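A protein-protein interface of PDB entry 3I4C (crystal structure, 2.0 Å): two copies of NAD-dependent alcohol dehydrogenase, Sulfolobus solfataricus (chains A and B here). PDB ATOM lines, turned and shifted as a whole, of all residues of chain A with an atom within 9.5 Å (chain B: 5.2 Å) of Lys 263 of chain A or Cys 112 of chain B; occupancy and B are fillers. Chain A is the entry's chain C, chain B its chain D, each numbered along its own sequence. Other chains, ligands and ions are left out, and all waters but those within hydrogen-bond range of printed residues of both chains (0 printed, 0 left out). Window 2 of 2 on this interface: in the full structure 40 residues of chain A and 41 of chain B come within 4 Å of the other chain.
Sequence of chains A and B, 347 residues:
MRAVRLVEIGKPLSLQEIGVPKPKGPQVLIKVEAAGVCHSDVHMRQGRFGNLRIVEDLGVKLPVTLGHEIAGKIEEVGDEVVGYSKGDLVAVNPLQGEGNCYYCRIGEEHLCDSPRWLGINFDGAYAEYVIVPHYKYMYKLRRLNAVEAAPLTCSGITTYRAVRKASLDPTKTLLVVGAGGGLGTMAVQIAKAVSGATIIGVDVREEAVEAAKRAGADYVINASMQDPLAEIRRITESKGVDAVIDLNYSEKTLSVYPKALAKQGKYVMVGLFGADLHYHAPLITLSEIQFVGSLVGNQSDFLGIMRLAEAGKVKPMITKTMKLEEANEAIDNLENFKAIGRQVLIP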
ATOM      1  N   LYS A 172      29.072 -15.987  -2.419  1.00  0.00           N
ATOM      2  CA  LYS A 172      28.248 -15.357  -3.440  1.00  0.00           C
ATOM      3  C   LYS A 172      27.725 -13.974  -3.097  1.00  0.00           C
ATOM      4  O   LYS A 172      27.744 -13.541  -1.941  1.00  0.00           O
ATOM      5  CB  LYS A 172      27.058 -16.253  -3.777  1.00  0.00           C
ATOM      6  CG  LYS A 172      27.451 -17.586  -4.353  1.00  0.00           C
ATOM      7  CD  LYS A 172      26.221 -18.381  -4.720  1.00  0.00           C
ATOM      8  CE  LYS A 172      26.598 -19.599  -5.552  1.00  0.00           C
ATOM      9  NZ  LYS A 172      25.375 -20.331  -5.983  1.00  0.00           N
ATOM     10  N   THR A 173      27.253 -13.278  -4.128  1.00  0.00           N
ATOM     11  CA  THR A 173      26.674 -11.953  -3.963  1.00  0.00           C
ATOM     12  C   THR A 173      25.264 -11.927  -4.550  1.00  0.00           C
ATOM     13  O   THR A 173      25.024 -12.384  -5.669  1.00  0.00           O
ATOM     14  CB  THR A 173      27.513 -10.862  -4.647  1.00  0.00           C
ATOM     15  OG1 THR A 173      28.736 -10.686  -3.922  1.00  0.00           O
ATOM     16  CG2 THR A 173      26.743  -9.542  -4.678  1.00  0.00           C
ATOM     17  N   SER A 238      33.507  -6.927 -11.904  1.00  0.00           N
ATOM     18  CA  SER A 238      33.087  -7.438 -13.200  1.00  0.00           C
ATOM     19  C   SER A 238      32.561  -8.866 -13.267  1.00  0.00           C
ATOM     20  O   SER A 238      32.217  -9.338 -14.346  1.00  0.00           O
ATOM     21  CB  SER A 238      34.207  -7.243 -14.226  1.00  0.00           C
ATOM     22  OG  SER A 238      34.409  -5.858 -14.488  1.00  0.00           O
ATOM     23  N   LYS A 239      32.479  -9.546 -12.126  1.00  0.00           N
ATOM     24  CA  LYS A 239      31.977 -10.916 -12.111  1.00  0.00           C
ATOM     25  C   LYS A 239      30.459 -10.946 -12.293  1.00  0.00           C
ATOM     26  O   LYS A 239      29.917 -11.839 -12.950  1.00  0.00           O
ATOM     27  CB  LYS A 239      32.333 -11.597 -10.789  1.00  0.00           C
ATOM     28  CG  LYS A 239      31.865 -13.044 -10.717  1.00  0.00           C
ATOM     29  CD  LYS A 239      31.872 -13.584  -9.298  1.00  0.00           C
ATOM     30  CE  LYS A 239      31.244 -14.972  -9.244  1.00  0.00           C
ATOM     31  NZ  LYS A 239      31.020 -15.435  -7.848  1.00  0.00           N
ATOM     32  N   GLY A 240      29.786  -9.955 -11.715  1.00  0.00           N
ATOM     33  CA  GLY A 240      28.338  -9.901 -11.785  1.00  0.00           C
ATOM     34  C   GLY A 240      27.822 -10.556 -10.518  1.00  0.00           C
ATOM     35  O   GLY A 240      28.627 -10.997  -9.700  1.00  0.00           O
ATOM     36  N   VAL A 241      26.504 -10.635 -10.357  1.00  0.00           N
ATOM     37  CA  VAL A 241      25.919 -11.237  -9.166  1.00  0.00           C
ATOM     38  C   VAL A 241      25.529 -12.702  -9.381  1.00  0.00           C
ATOM     39  O   VAL A 241      25.177 -13.120 -10.493  1.00  0.00           O
ATOM     40  CB  VAL A 241      24.693 -10.416  -8.686  1.00  0.00           C
ATOM     41  CG1 VAL A 241      25.148  -9.019  -8.280  1.00  0.00           C
ATOM     42  CG2 VAL A 241      23.645 -10.324  -9.792  1.00  0.00           C
ATOM     43  N   ASP A 242      25.595 -13.481  -8.309  1.00  0.00           N
ATOM     44  CA  ASP A 242      25.295 -14.906  -8.388  1.00  0.00           C
ATOM     45  C   ASP A 242      23.807 -15.194  -8.332  1.00  0.00           C
ATOM     46  O   ASP A 242      23.360 -16.290  -8.679  1.00  0.00           O
ATOM     47  CB  ASP A 242      26.035 -15.627  -7.266  1.00  0.00           C
ATOM     48  CG  ASP A 242      27.529 -15.376  -7.318  1.00  0.00           C
ATOM     49  OD1 ASP A 242      28.206 -15.982  -8.175  1.00  0.00           O
ATOM     50  OD2 ASP A 242      28.030 -14.560  -6.513  1.00  0.00           O
ATOM     51  N   ALA A 243      23.046 -14.199  -7.895  1.00  0.00           N
ATOM     52  CA  ALA A 243      21.607 -14.330  -7.822  1.00  0.00           C
ATOM     53  C   ALA A 243      20.956 -12.962  -7.791  1.00  0.00           C
ATOM     54  O   ALA A 243      21.542 -11.978  -7.325  1.00  0.00           O
ATOM     55  CB  ALA A 243      21.201 -15.143  -6.568  1.00  0.00           C
ATOM     56  N   PRO A 258      18.826  -8.864 -15.717  1.00  0.00           N
ATOM     57  CA  PRO A 258      19.466 -10.143 -16.028  1.00  0.00           C
ATOM     58  C   PRO A 258      20.884  -9.897 -16.554  1.00  0.00           C
ATOM     59  O   PRO A 258      21.733 -10.781 -16.512  1.00  0.00           O
ATOM     60  CB  PRO A 258      18.550 -10.743 -17.092  1.00  0.00           C
ATOM     61  CG  PRO A 258      17.202 -10.224 -16.682  1.00  0.00           C
ATOM     62  CD  PRO A 258      17.513  -8.763 -16.376  1.00  0.00           C
ATOM     63  N   LYS A 259      21.139  -8.686 -17.044  1.00  0.00           N
ATOM     64  CA  LYS A 259      22.462  -8.352 -17.558  1.00  0.00           C
ATOM     65  C   LYS A 259      23.515  -8.312 -16.452  1.00  0.00           C
ATOM     66  O   LYS A 259      24.713  -8.377 -16.732  1.00  0.00           O
ATOM     67  CB  LYS A 259      22.442  -7.001 -18.283  1.00  0.00           C
ATOM     68  CG  LYS A 259      21.554  -6.959 -19.519  1.00  0.00           C
ATOM     69  CD  LYS A 259      21.596  -5.583 -20.181  1.00  0.00           C
ATOM     70  CE  LYS A 259      20.634  -5.502 -21.354  1.00  0.00           C
ATOM     71  NZ  LYS A 259      20.631  -4.148 -21.965  1.00  0.00           N
ATOM     72  N   ALA A 260      23.075  -8.214 -15.202  1.00  0.00           N
ATOM     73  CA  ALA A 260      24.002  -8.159 -14.070  1.00  0.00           C
ATOM     74  C   ALA A 260      24.389  -9.552 -13.560  1.00  0.00           C
ATOM     75  O   ALA A 260      25.254  -9.689 -12.691  1.00  0.00           O
ATOM     76  CB  ALA A 260      23.382  -7.343 -12.942  1.00  0.00           C
ATOM     77  N   LEU A 261      23.755 -10.587 -14.106  1.00  0.00           N
ATOM     78  CA  LEU A 261      24.036 -11.956 -13.683  1.00  0.00           C
ATOM     79  C   LEU A 261      25.439 -12.449 -13.998  1.00  0.00           C
ATOM     80  O   LEU A 261      25.977 -12.211 -15.082  1.00  0.00           O
ATOM     81  CB  LEU A 261      23.043 -12.930 -14.321  1.00  0.00           C
ATOM     82  CG  LEU A 261      21.595 -12.954 -13.833  1.00  0.00           C
ATOM     83  CD1 LEU A 261      20.766 -13.850 -14.757  1.00  0.00           C
ATOM     84  CD2 LEU A 261      21.546 -13.479 -12.399  1.00  0.00           C
ATOM     85  N   ALA A 262      26.028 -13.154 -13.042  1.00  0.00           N
ATOM     86  CA  ALA A 262      27.348 -13.738 -13.237  1.00  0.00           C
ATOM     87  C   ALA A 262      27.104 -15.107 -13.868  1.00  0.00           C
ATOM     88  O   ALA A 262      25.960 -15.525 -14.017  1.00  0.00           O
ATOM     89  CB  ALA A 262      28.041 -13.896 -11.900  1.00  0.00           C
ATOM     90  N   LYS A 263      28.169 -15.798 -14.262  1.00  0.00           N
ATOM     91  CA  LYS A 263      28.018 -17.133 -14.829  1.00  0.00           C
ATOM     92  C   LYS A 263      27.403 -17.994 -13.719  1.00  0.00           C
ATOM     93  O   LYS A 263      27.781 -17.864 -12.554  1.00  0.00           O
ATOM     94  CB  LYS A 263      29.387 -17.664 -15.276  1.00  0.00           C
ATOM     95  CG  LYS A 263      29.919 -16.940 -16.524  1.00  0.00           C
ATOM     96  CD  LYS A 263      31.306 -17.412 -16.942  1.00  0.00           C
ATOM     97  CE  LYS A 263      32.398 -16.775 -16.092  1.00  0.00           C
ATOM     98  NZ  LYS A 263      33.757 -17.251 -16.488  1.00  0.00           N
ATOM     99  N   GLN A 264      26.453 -18.852 -14.087  1.00  0.00           N
ATOM    100  CA  GLN A 264      25.708 -19.705 -13.150  1.00  0.00           C
ATOM    101  C   GLN A 264      24.761 -18.891 -12.259  1.00  0.00           C
ATOM    102  O   GLN A 264      24.244 -19.402 -11.264  1.00  0.00           O
ATOM    103  CB  GLN A 264      26.636 -20.555 -12.261  1.00  0.00           C
ATOM    104  CG  GLN A 264      27.273 -21.746 -12.971  1.00  0.00           C
ATOM    105  CD  GLN A 264      27.944 -22.751 -12.031  1.00  0.00           C
ATOM    106  OE1 GLN A 264      28.543 -22.384 -11.013  1.00  0.00           O
ATOM    107  NE2 GLN A 264      27.868 -24.031 -12.394  1.00  0.00           N
ATOM    108  N   GLY A 265      24.534 -17.629 -12.617  1.00  0.00           N
ATOM    109  CA  GLY A 265      23.643 -16.790 -11.834  1.00  0.00           C
ATOM    110  C   GLY A 265      22.188 -17.228 -11.929  1.00  0.00           C
ATOM    111  O   GLY A 265      21.739 -17.737 -12.964  1.00  0.00           O
ATOM    112  N   LYS A 266      21.450 -17.046 -10.840  1.00  0.00           N
ATOM    113  CA  LYS A 266      20.048 -17.421 -10.805  1.00  0.00           C
ATOM    114  C   LYS A 266      19.193 -16.177 -10.648  1.00  0.00           C
ATOM    115  O   LYS A 266      19.375 -15.388  -9.712  1.00  0.00           O
ATOM    116  CB  LYS A 266      19.782 -18.399  -9.655  1.00  0.00           C
ATOM    117  CG  LYS A 266      20.514 -19.732  -9.796  1.00  0.00           C
ATOM    118  CD  LYS A 266      20.015 -20.754  -8.773  1.00  0.00           C
ATOM    119  CE  LYS A 266      20.719 -22.097  -8.955  1.00  0.00           C
ATOM    120  NZ  LYS A 266      20.056 -23.228  -8.218  1.00  0.00           N
ATOM    121  N   LEU A 283      23.050 -16.481 -24.596  1.00  0.00           N
ATOM    122  CA  LEU A 283      23.589 -15.916 -23.367  1.00  0.00           C
ATOM    123  C   LEU A 283      23.259 -16.842 -22.203  1.00  0.00           C
ATOM    124  O   LEU A 283      24.018 -16.940 -21.241  1.00  0.00           O
ATOM    125  CB  LEU A 283      23.001 -14.533 -23.114  1.00  0.00           C
ATOM    126  CG  LEU A 283      23.271 -13.520 -24.235  1.00  0.00           C
ATOM    127  CD1 LEU A 283      22.559 -12.223 -23.917  1.00  0.00           C
ATOM    128  CD2 LEU A 283      24.770 -13.292 -24.394  1.00  0.00           C
ATOM    129  N   ILE A 284      22.133 -17.539 -22.299  1.00  0.00           N
ATOM    130  CA  ILE A 284      21.719 -18.442 -21.226  1.00  0.00           C
ATOM    131  C   ILE A 284      22.577 -19.696 -21.170  1.00  0.00           C
ATOM    132  O   ILE A 284      23.000 -20.120 -20.095  1.00  0.00           O
ATOM    133  CB  ILE A 284      20.249 -18.857 -21.384  1.00  0.00           C
ATOM    134  CG1 ILE A 284      19.370 -17.604 -21.367  1.00  0.00           C
ATOM    135  CG2 ILE A 284      19.848 -19.826 -20.256  1.00  0.00           C
ATOM    136  CD1 ILE A 284      17.901 -17.879 -21.574  1.00  0.00           C
ATOM    137  N   THR A 285      22.845 -20.288 -22.327  1.00  0.00           N
ATOM    138  CA  THR A 285      23.643 -21.499 -22.370  1.00  0.00           C
ATOM    139  C   THR A 285      25.107 -21.245 -22.081  1.00  0.00           C
ATOM    140  O   THR A 285      25.739 -22.015 -21.358  1.00  0.00           O
ATOM    141  CB  THR A 285      23.564 -22.212 -23.737  1.00  0.00           C
ATOM    142  OG1 THR A 285      24.118 -21.362 -24.747  1.00  0.00           O
ATOM    143  CG2 THR A 285      22.124 -22.562 -24.076  1.00  0.00           C
ATOM    144  N   LEU A 286      25.658 -20.178 -22.652  1.00  0.00           N
ATOM    145  CA  LEU A 286      27.062 -19.858 -22.433  1.00  0.00           C
ATOM    146  C   LEU A 286      27.393 -19.603 -20.973  1.00  0.00           C
ATOM    147  O   LEU A 286      28.478 -19.935 -20.509  1.00  0.00           O
ATOM    148  CB  LEU A 286      27.468 -18.626 -23.237  1.00  0.00           C
ATOM    149  CG  LEU A 286      27.606 -18.847 -24.743  1.00  0.00           C
ATOM    150  CD1 LEU A 286      27.795 -17.504 -25.455  1.00  0.00           C
ATOM    151  CD2 LEU A 286      28.788 -19.762 -24.998  1.00  0.00           C
ATOM    152  N   SER A 287      26.469 -19.003 -20.241  1.00  0.00           N
ATOM    153  CA  SER A 287      26.751 -18.702 -18.848  1.00  0.00           C
ATOM    154  C   SER A 287      26.081 -19.623 -17.852  1.00  0.00           C
ATOM    155  O   SER A 287      26.276 -19.472 -16.647  1.00  0.00           O
ATOM    156  CB  SER A 287      26.376 -17.254 -18.531  1.00  0.00           C
ATOM    157  OG  SER A 287      27.336 -16.365 -19.076  1.00  0.00           O
ATOM    158  N   GLU A 288      25.306 -20.583 -18.347  1.00  0.00           N
ATOM    159  CA  GLU A 288      24.597 -21.499 -17.459  1.00  0.00           C
ATOM    160  C   GLU A 288      23.691 -20.729 -16.497  1.00  0.00           C
ATOM    161  O   GLU A 288      23.516 -21.139 -15.348  1.00  0.00           O
ATOM    162  CB  GLU A 288      25.584 -22.372 -16.643  1.00  0.00           C
ATOM    163  CG  GLU A 288      26.021 -23.659 -17.334  1.00  0.00           C
ATOM    164  CD  GLU A 288      26.789 -24.639 -16.432  1.00  0.00           C
ATOM    165  OE1 GLU A 288      26.507 -24.721 -15.214  1.00  0.00           O
ATOM    166  OE2 GLU A 288      27.666 -25.364 -16.957  1.00  0.00           O
ATOM    167  N   ILE A 289      23.100 -19.624 -16.942  1.00  0.00           N
ATOM    168  CA  ILE A 289      22.232 -18.908 -16.023  1.00  0.00           C
ATOM    169  C   ILE A 289      20.873 -19.588 -15.942  1.00  0.00           C
ATOM    170  O   ILE A 289      20.541 -20.450 -16.760  1.00  0.00           O
ATOM    171  CB  ILE A 289      22.063 -17.415 -16.404  1.00  0.00           C
ATOM    172  CG1 ILE A 289      21.372 -17.280 -17.749  1.00  0.00           C
ATOM    173  CG2 ILE A 289      23.435 -16.723 -16.412  1.00  0.00           C
ATOM    174  CD1 ILE A 289      21.067 -15.836 -18.128  1.00  0.00           C
ATOM    175  N   GLN A 290      20.103 -19.224 -14.929  1.00  0.00           N
ATOM    176  CA  GLN A 290      18.785 -19.798 -14.745  1.00  0.00           C
ATOM    177  C   GLN A 290      17.789 -18.708 -14.399  1.00  0.00           C
ATOM    178  O   GLN A 290      18.108 -17.771 -13.660  1.00  0.00           O
ATOM    179  CB  GLN A 290      18.794 -20.833 -13.604  1.00  0.00           C
ATOM    180  CG  GLN A 290      19.734 -22.012 -13.799  1.00  0.00           C
ATOM    181  CD  GLN A 290      19.692 -23.000 -12.636  1.00  0.00           C
ATOM    182  OE1 GLN A 290      18.625 -23.299 -12.088  1.00  0.00           O
ATOM    183  NE2 GLN A 290      20.855 -23.522 -12.265  1.00  0.00           N
ATOM    184  N   GLY B  97      40.642 -25.319 -16.784  1.00  0.00           N
ATOM    185  CA  GLY B  97      40.744 -24.025 -16.129  1.00  0.00           C
ATOM    186  C   GLY B  97      42.118 -23.670 -15.585  1.00  0.00           C
ATOM    187  O   GLY B  97      42.919 -24.550 -15.261  1.00  0.00           O
ATOM    188  N   GLU B  98      42.388 -22.370 -15.482  1.00  0.00           N
ATOM    189  CA  GLU B  98      43.671 -21.888 -14.984  1.00  0.00           C
ATOM    190  C   GLU B  98      43.819 -22.092 -13.471  1.00  0.00           C
ATOM    191  O   GLU B  98      44.930 -22.071 -12.940  1.00  0.00           O
ATOM    192  CB  GLU B  98      43.865 -20.412 -15.365  1.00  0.00           C
ATOM    193  CG  GLU B  98      42.683 -19.504 -15.049  1.00  0.00           C
ATOM    194  CD  GLU B  98      42.481 -19.320 -13.564  1.00  0.00           C
ATOM    195  OE1 GLU B  98      43.468 -18.982 -12.876  1.00  0.00           O
ATOM    196  OE2 GLU B  98      41.346 -19.497 -13.073  1.00  0.00           O
ATOM    197  N   GLY B  99      42.699 -22.281 -12.777  1.00  0.00           N
ATOM    198  CA  GLY B  99      42.758 -22.543 -11.348  1.00  0.00           C
ATOM    199  C   GLY B  99      42.507 -21.453 -10.316  1.00  0.00           C
ATOM    200  O   GLY B  99      41.964 -21.732  -9.235  1.00  0.00           O
ATOM    201  N   CYS B 101      40.601 -18.442 -10.686  1.00  0.00           N
ATOM    202  CA  CYS B 101      39.302 -17.780 -10.659  1.00  0.00           C
ATOM    203  C   CYS B 101      38.278 -18.484  -9.778  1.00  0.00           C
ATOM    204  O   CYS B 101      38.477 -19.618  -9.340  1.00  0.00           O
ATOM    205  CB  CYS B 101      38.746 -17.588 -12.081  1.00  0.00           C
ATOM    206  SG  CYS B 101      37.951 -19.033 -12.875  1.00  0.00           S
ATOM    207  N   TYR B 103      35.264 -19.736 -10.416  1.00  0.00           N
ATOM    208  CA  TYR B 103      34.708 -20.960 -10.960  1.00  0.00           C
ATOM    209  C   TYR B 103      35.637 -22.158 -10.847  1.00  0.00           C
ATOM    210  O   TYR B 103      35.174 -23.278 -10.596  1.00  0.00           O
ATOM    211  CB  TYR B 103      34.252 -20.669 -12.391  1.00  0.00           C
ATOM    212  CG  TYR B 103      33.154 -19.620 -12.361  1.00  0.00           C
ATOM    213  CD1 TYR B 103      31.839 -19.972 -12.031  1.00  0.00           C
ATOM    214  CD2 TYR B 103      33.446 -18.262 -12.532  1.00  0.00           C
ATOM    215  CE1 TYR B 103      30.854 -19.012 -11.865  1.00  0.00           C
ATOM    216  CE2 TYR B 103      32.460 -17.285 -12.363  1.00  0.00           C
ATOM    217  CZ  TYR B 103      31.170 -17.668 -12.028  1.00  0.00           C
ATOM    218  OH  TYR B 103      30.193 -16.716 -11.844  1.00  0.00           O
ATOM    219  N   CYS B 104      36.940 -21.931 -11.002  1.00  0.00           N
ATOM    220  CA  CYS B 104      37.904 -23.019 -10.863  1.00  0.00           C
ATOM    221  C   CYS B 104      37.930 -23.430  -9.390  1.00  0.00           C
ATOM    222  O   CYS B 104      37.937 -24.617  -9.061  1.00  0.00           O
ATOM    223  CB  CYS B 104      39.311 -22.573 -11.296  1.00  0.00           C
ATOM    224  SG  CYS B 104      39.588 -22.545 -13.101  1.00  0.00           S
ATOM    225  N   GLU B 108      33.991 -25.744 -10.905  1.00  0.00           N
ATOM    226  CA  GLU B 108      33.267 -25.572 -12.159  1.00  0.00           C
ATOM    227  C   GLU B 108      34.247 -24.982 -13.183  1.00  0.00           C
ATOM    228  O   GLU B 108      33.962 -23.965 -13.811  1.00  0.00           O
ATOM    229  CB  GLU B 108      32.106 -24.602 -11.937  1.00  0.00           C
ATOM    230  CG  GLU B 108      31.135 -25.010 -10.822  1.00  0.00           C
ATOM    231  CD  GLU B 108      30.337 -26.244 -11.181  1.00  0.00           C
ATOM    232  OE1 GLU B 108      29.686 -26.237 -12.242  1.00  0.00           O
ATOM    233  OE2 GLU B 108      30.362 -27.226 -10.412  1.00  0.00           O
ATOM    234  N   GLU B 109      35.390 -25.638 -13.357  1.00  0.00           N
ATOM    235  CA  GLU B 109      36.424 -25.141 -14.255  1.00  0.00           C
ATOM    236  C   GLU B 109      36.031 -24.933 -15.713  1.00  0.00           C
ATOM    237  O   GLU B 109      36.701 -24.195 -16.427  1.00  0.00           O
ATOM    238  CB  GLU B 109      37.666 -26.034 -14.175  1.00  0.00           C
ATOM    239  CG  GLU B 109      37.528 -27.414 -14.806  1.00  0.00           C
ATOM    240  CD  GLU B 109      38.831 -28.172 -14.774  1.00  0.00           C
ATOM    241  OE1 GLU B 109      39.836 -27.641 -15.296  1.00  0.00           O
ATOM    242  OE2 GLU B 109      38.862 -29.295 -14.232  1.00  0.00           O
ATOM    243  N   HIS B 110      34.961 -25.568 -16.168  1.00  0.00           N
ATOM    244  CA  HIS B 110      34.550 -25.375 -17.553  1.00  0.00           C
ATOM    245  C   HIS B 110      34.037 -23.946 -17.714  1.00  0.00           C
ATOM    246  O   HIS B 110      33.939 -23.436 -18.825  1.00  0.00           O
ATOM    247  CB  HIS B 110      33.465 -26.375 -17.930  1.00  0.00           C
ATOM    248  CG  HIS B 110      32.253 -26.305 -17.052  1.00  0.00           C
ATOM    249  ND1 HIS B 110      32.290 -26.609 -15.711  1.00  0.00           N
ATOM    250  CD2 HIS B 110      30.971 -25.976 -17.333  1.00  0.00           C
ATOM    251  CE1 HIS B 110      31.079 -26.474 -15.199  1.00  0.00           C
ATOM    252  NE2 HIS B 110      30.261 -26.090 -16.161  1.00  0.00           N
ATOM    253  N   LEU B 111      33.710 -23.298 -16.598  1.00  0.00           N
ATOM    254  CA  LEU B 111      33.232 -21.918 -16.649  1.00  0.00           C
ATOM    255  C   LEU B 111      34.350 -20.959 -16.245  1.00  0.00           C
ATOM    256  O   LEU B 111      34.099 -19.811 -15.885  1.00  0.00           O
ATOM    257  CB  LEU B 111      32.023 -21.722 -15.726  1.00  0.00           C
ATOM    258  CG  LEU B 111      30.756 -22.487 -16.121  1.00  0.00           C
ATOM    259  CD1 LEU B 111      29.673 -22.260 -15.078  1.00  0.00           C
ATOM    260  CD2 LEU B 111      30.280 -22.019 -17.489  1.00  0.00           C
ATOM    261  N   CYS B 112      35.581 -21.449 -16.290  1.00  0.00           N
ATOM    262  CA  CYS B 112      36.751 -20.644 -15.953  1.00  0.00           C
ATOM    263  C   CYS B 112      36.738 -19.320 -16.718  1.00  0.00           C
ATOM    264  O   CYS B 112      36.286 -19.268 -17.867  1.00  0.00           O
ATOM    265  CB  CYS B 112      38.031 -21.409 -16.307  1.00  0.00           C
ATOM    266  SG  CYS B 112      39.573 -20.460 -16.084  1.00  0.00           S
ATOM    267  N   ASP B 113      37.231 -18.259 -16.081  1.00  0.00           N
ATOM    268  CA  ASP B 113      37.292 -16.935 -16.708  1.00  0.00           C
ATOM    269  C   ASP B 113      38.324 -16.873 -17.860  1.00  0.00           C
ATOM    270  O   ASP B 113      38.168 -16.091 -18.800  1.00  0.00           O
ATOM    271  CB  ASP B 113      37.652 -15.855 -15.677  1.00  0.00           C
ATOM    272  CG  ASP B 113      36.527 -15.567 -14.683  1.00  0.00           C
ATOM    273  OD1 ASP B 113      35.335 -15.712 -15.034  1.00  0.00           O
ATOM    274  OD2 ASP B 113      36.845 -15.158 -13.546  1.00  0.00           O
ATOM    275  N   SER B 114      39.372 -17.685 -17.770  1.00  0.00           N
ATOM    276  CA  SER B 114      40.430 -17.722 -18.784  1.00  0.00           C
ATOM    277  C   SER B 114      40.867 -19.171 -18.954  1.00  0.00           C
ATOM    278  O   SER B 114      41.951 -19.553 -18.526  1.00  0.00           O
ATOM    279  CB  SER B 114      41.640 -16.902 -18.320  1.00  0.00           C
ATOM    280  OG  SER B 114      41.248 -15.671 -17.740  1.00  0.00           O
ATOM    281  N   PRO B 115      40.032 -19.995 -19.593  1.00  0.00           N
ATOM    282  CA  PRO B 115      40.353 -21.410 -19.797  1.00  0.00           C
ATOM    283  C   PRO B 115      41.370 -21.717 -20.895  1.00  0.00           C
ATOM    284  O   PRO B 115      41.652 -20.889 -21.759  1.00  0.00           O
ATOM    285  CB  PRO B 115      38.993 -22.013 -20.121  1.00  0.00           C
ATOM    286  CG  PRO B 115      38.371 -20.925 -20.941  1.00  0.00           C
ATOM    287  CD  PRO B 115      38.712 -19.668 -20.157  1.00  0.00           C
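Among the printed residues, merely in contact across the chains: Gln 264 of chain A with Leu 111 of chain B (3.2 Å), Lys 239 of chain A with Tyr 103 of chain B (3.3 Å), Lys 263 of chain A with Cys 112 of chain B (3.5 Å), Ala 262 of chain A with Tyr 103 of chain B (3.5 Å) and Glu 288 of chain A with Leu 111 of chain B (3.98 Å).
The side-chain amino group of Lys 263 of chain A is in salt-bridge range of the side-chain carboxylate of Asp 113 of chain B, 2.6 Å away. NZ of Lys 263 of chain A sits at hydrogen-bond distance from O of Leu 111 of chain B, 2.7 Å away. The side-chain carboxylate of Glu 288 of chain A sits at hydrogen-bond distance from a ring nitrogen (NE2) of His 110 of chain B, 2.8 Å away. The side-chain carboxylate of Glu 108 of chain B lies within hydrogen-bond range of the side-chain amide nitrogen of Gln 264 of chain A. The side-chain hydroxyl (OH) of Tyr 103 of chain B is in hydrogen-bond range of the backbone carbonyl oxygen (O) of Lys 263 of chain A (2.8 Å).
Printed residues of chain B within 4 Å of Lys 263 of chain A: Tyr 103 (2.8 Å), Leu 111 (2.7 Å), Cys 112 (3.5 Å) and Asp 113 (2.6 Å). Of chain A, only Lys 263 (2.7 Å), Gln 264 (3.2 Å) and Glu 288 (3.98 Å) come within 4 Å of Leu 111 of chain B. Of the printed residues of chain A, Asp 113 of chain B touches Lys 263. Ser 114 of chain B touches none of the printed residues of chain A. Of the printed residues of chain B, Gln 264 of chain A touches Glu 108 (2.9 Å) and Leu 111 (3.2 Å). Of the printed residues of chain A, His 110 of chain B touches Glu 288 (2.8 Å). Printed residues of chain A within 4 Å of Tyr 103 of chain B: Lys 239 (3.3 Å), Ala 262 (3.5 Å) and Lys 263 (2.8 Å). Printed residues of chain B within 4 Å of Lys 239 of chain A: Tyr 103. The nearest printed residue of chain B that does not touch Lys 263 of chain A is Ser 114 of chain B (5.8 Å). The nearest residue of chain A that does not touch Cys 112 of chain B is Leu 286 of chain A (8.3 Å). The nearest printed residue of chain A that does not touch Tyr 103 of chain B is Gln 264 of chain A (4.2 Å).
No position is printed for both chains.
Printed residues of chain B that touch a printed residue of chain A: Tyr 103, Glu 108, His 110, Leu 111, Cys 112 and Asp 113. Hydrophobic or aromatic side chains of chain A that line the printed part of chain B: Ala 262. Among the printed residues, 10 pairs touch across the chains. Among the printed residues, Asp or Glu carboxylates within 4 Å of a Lys or Arg side-chain nitrogen of the other chain: Lys 263 of chain A with Asp 113 of chain B.
N of Glu 108 of chain B lies within hydrogen-bond range of O of Tyr 103 of chain B, at 2.8 Å. N of Ala 262 of chain A lies within hydrogen-bond range of O of Val 241 of chain A, 2.7 Å away. The side-chain amide nitrogen (NE2) of Gln 264 of chain A sits at hydrogen-bond distance from the side-chain carboxylate (OE1) of Glu 288 of chain A (3.2 Å). The backbone NH (N) of Gln 264 of chain A sits at hydrogen-bond distance from the backbone carbonyl oxygen (O) of Ser 287 of chain A (2.6 Å). N of Ser 114 of chain B sits close to SG of Cys 112 of chain B, 3.3 Å away. The side-chain sulfur (SG) of Cys 101 of chain B lies close to the backbone NH (N) of Asp 113 of chain B, 3.4 Å away.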
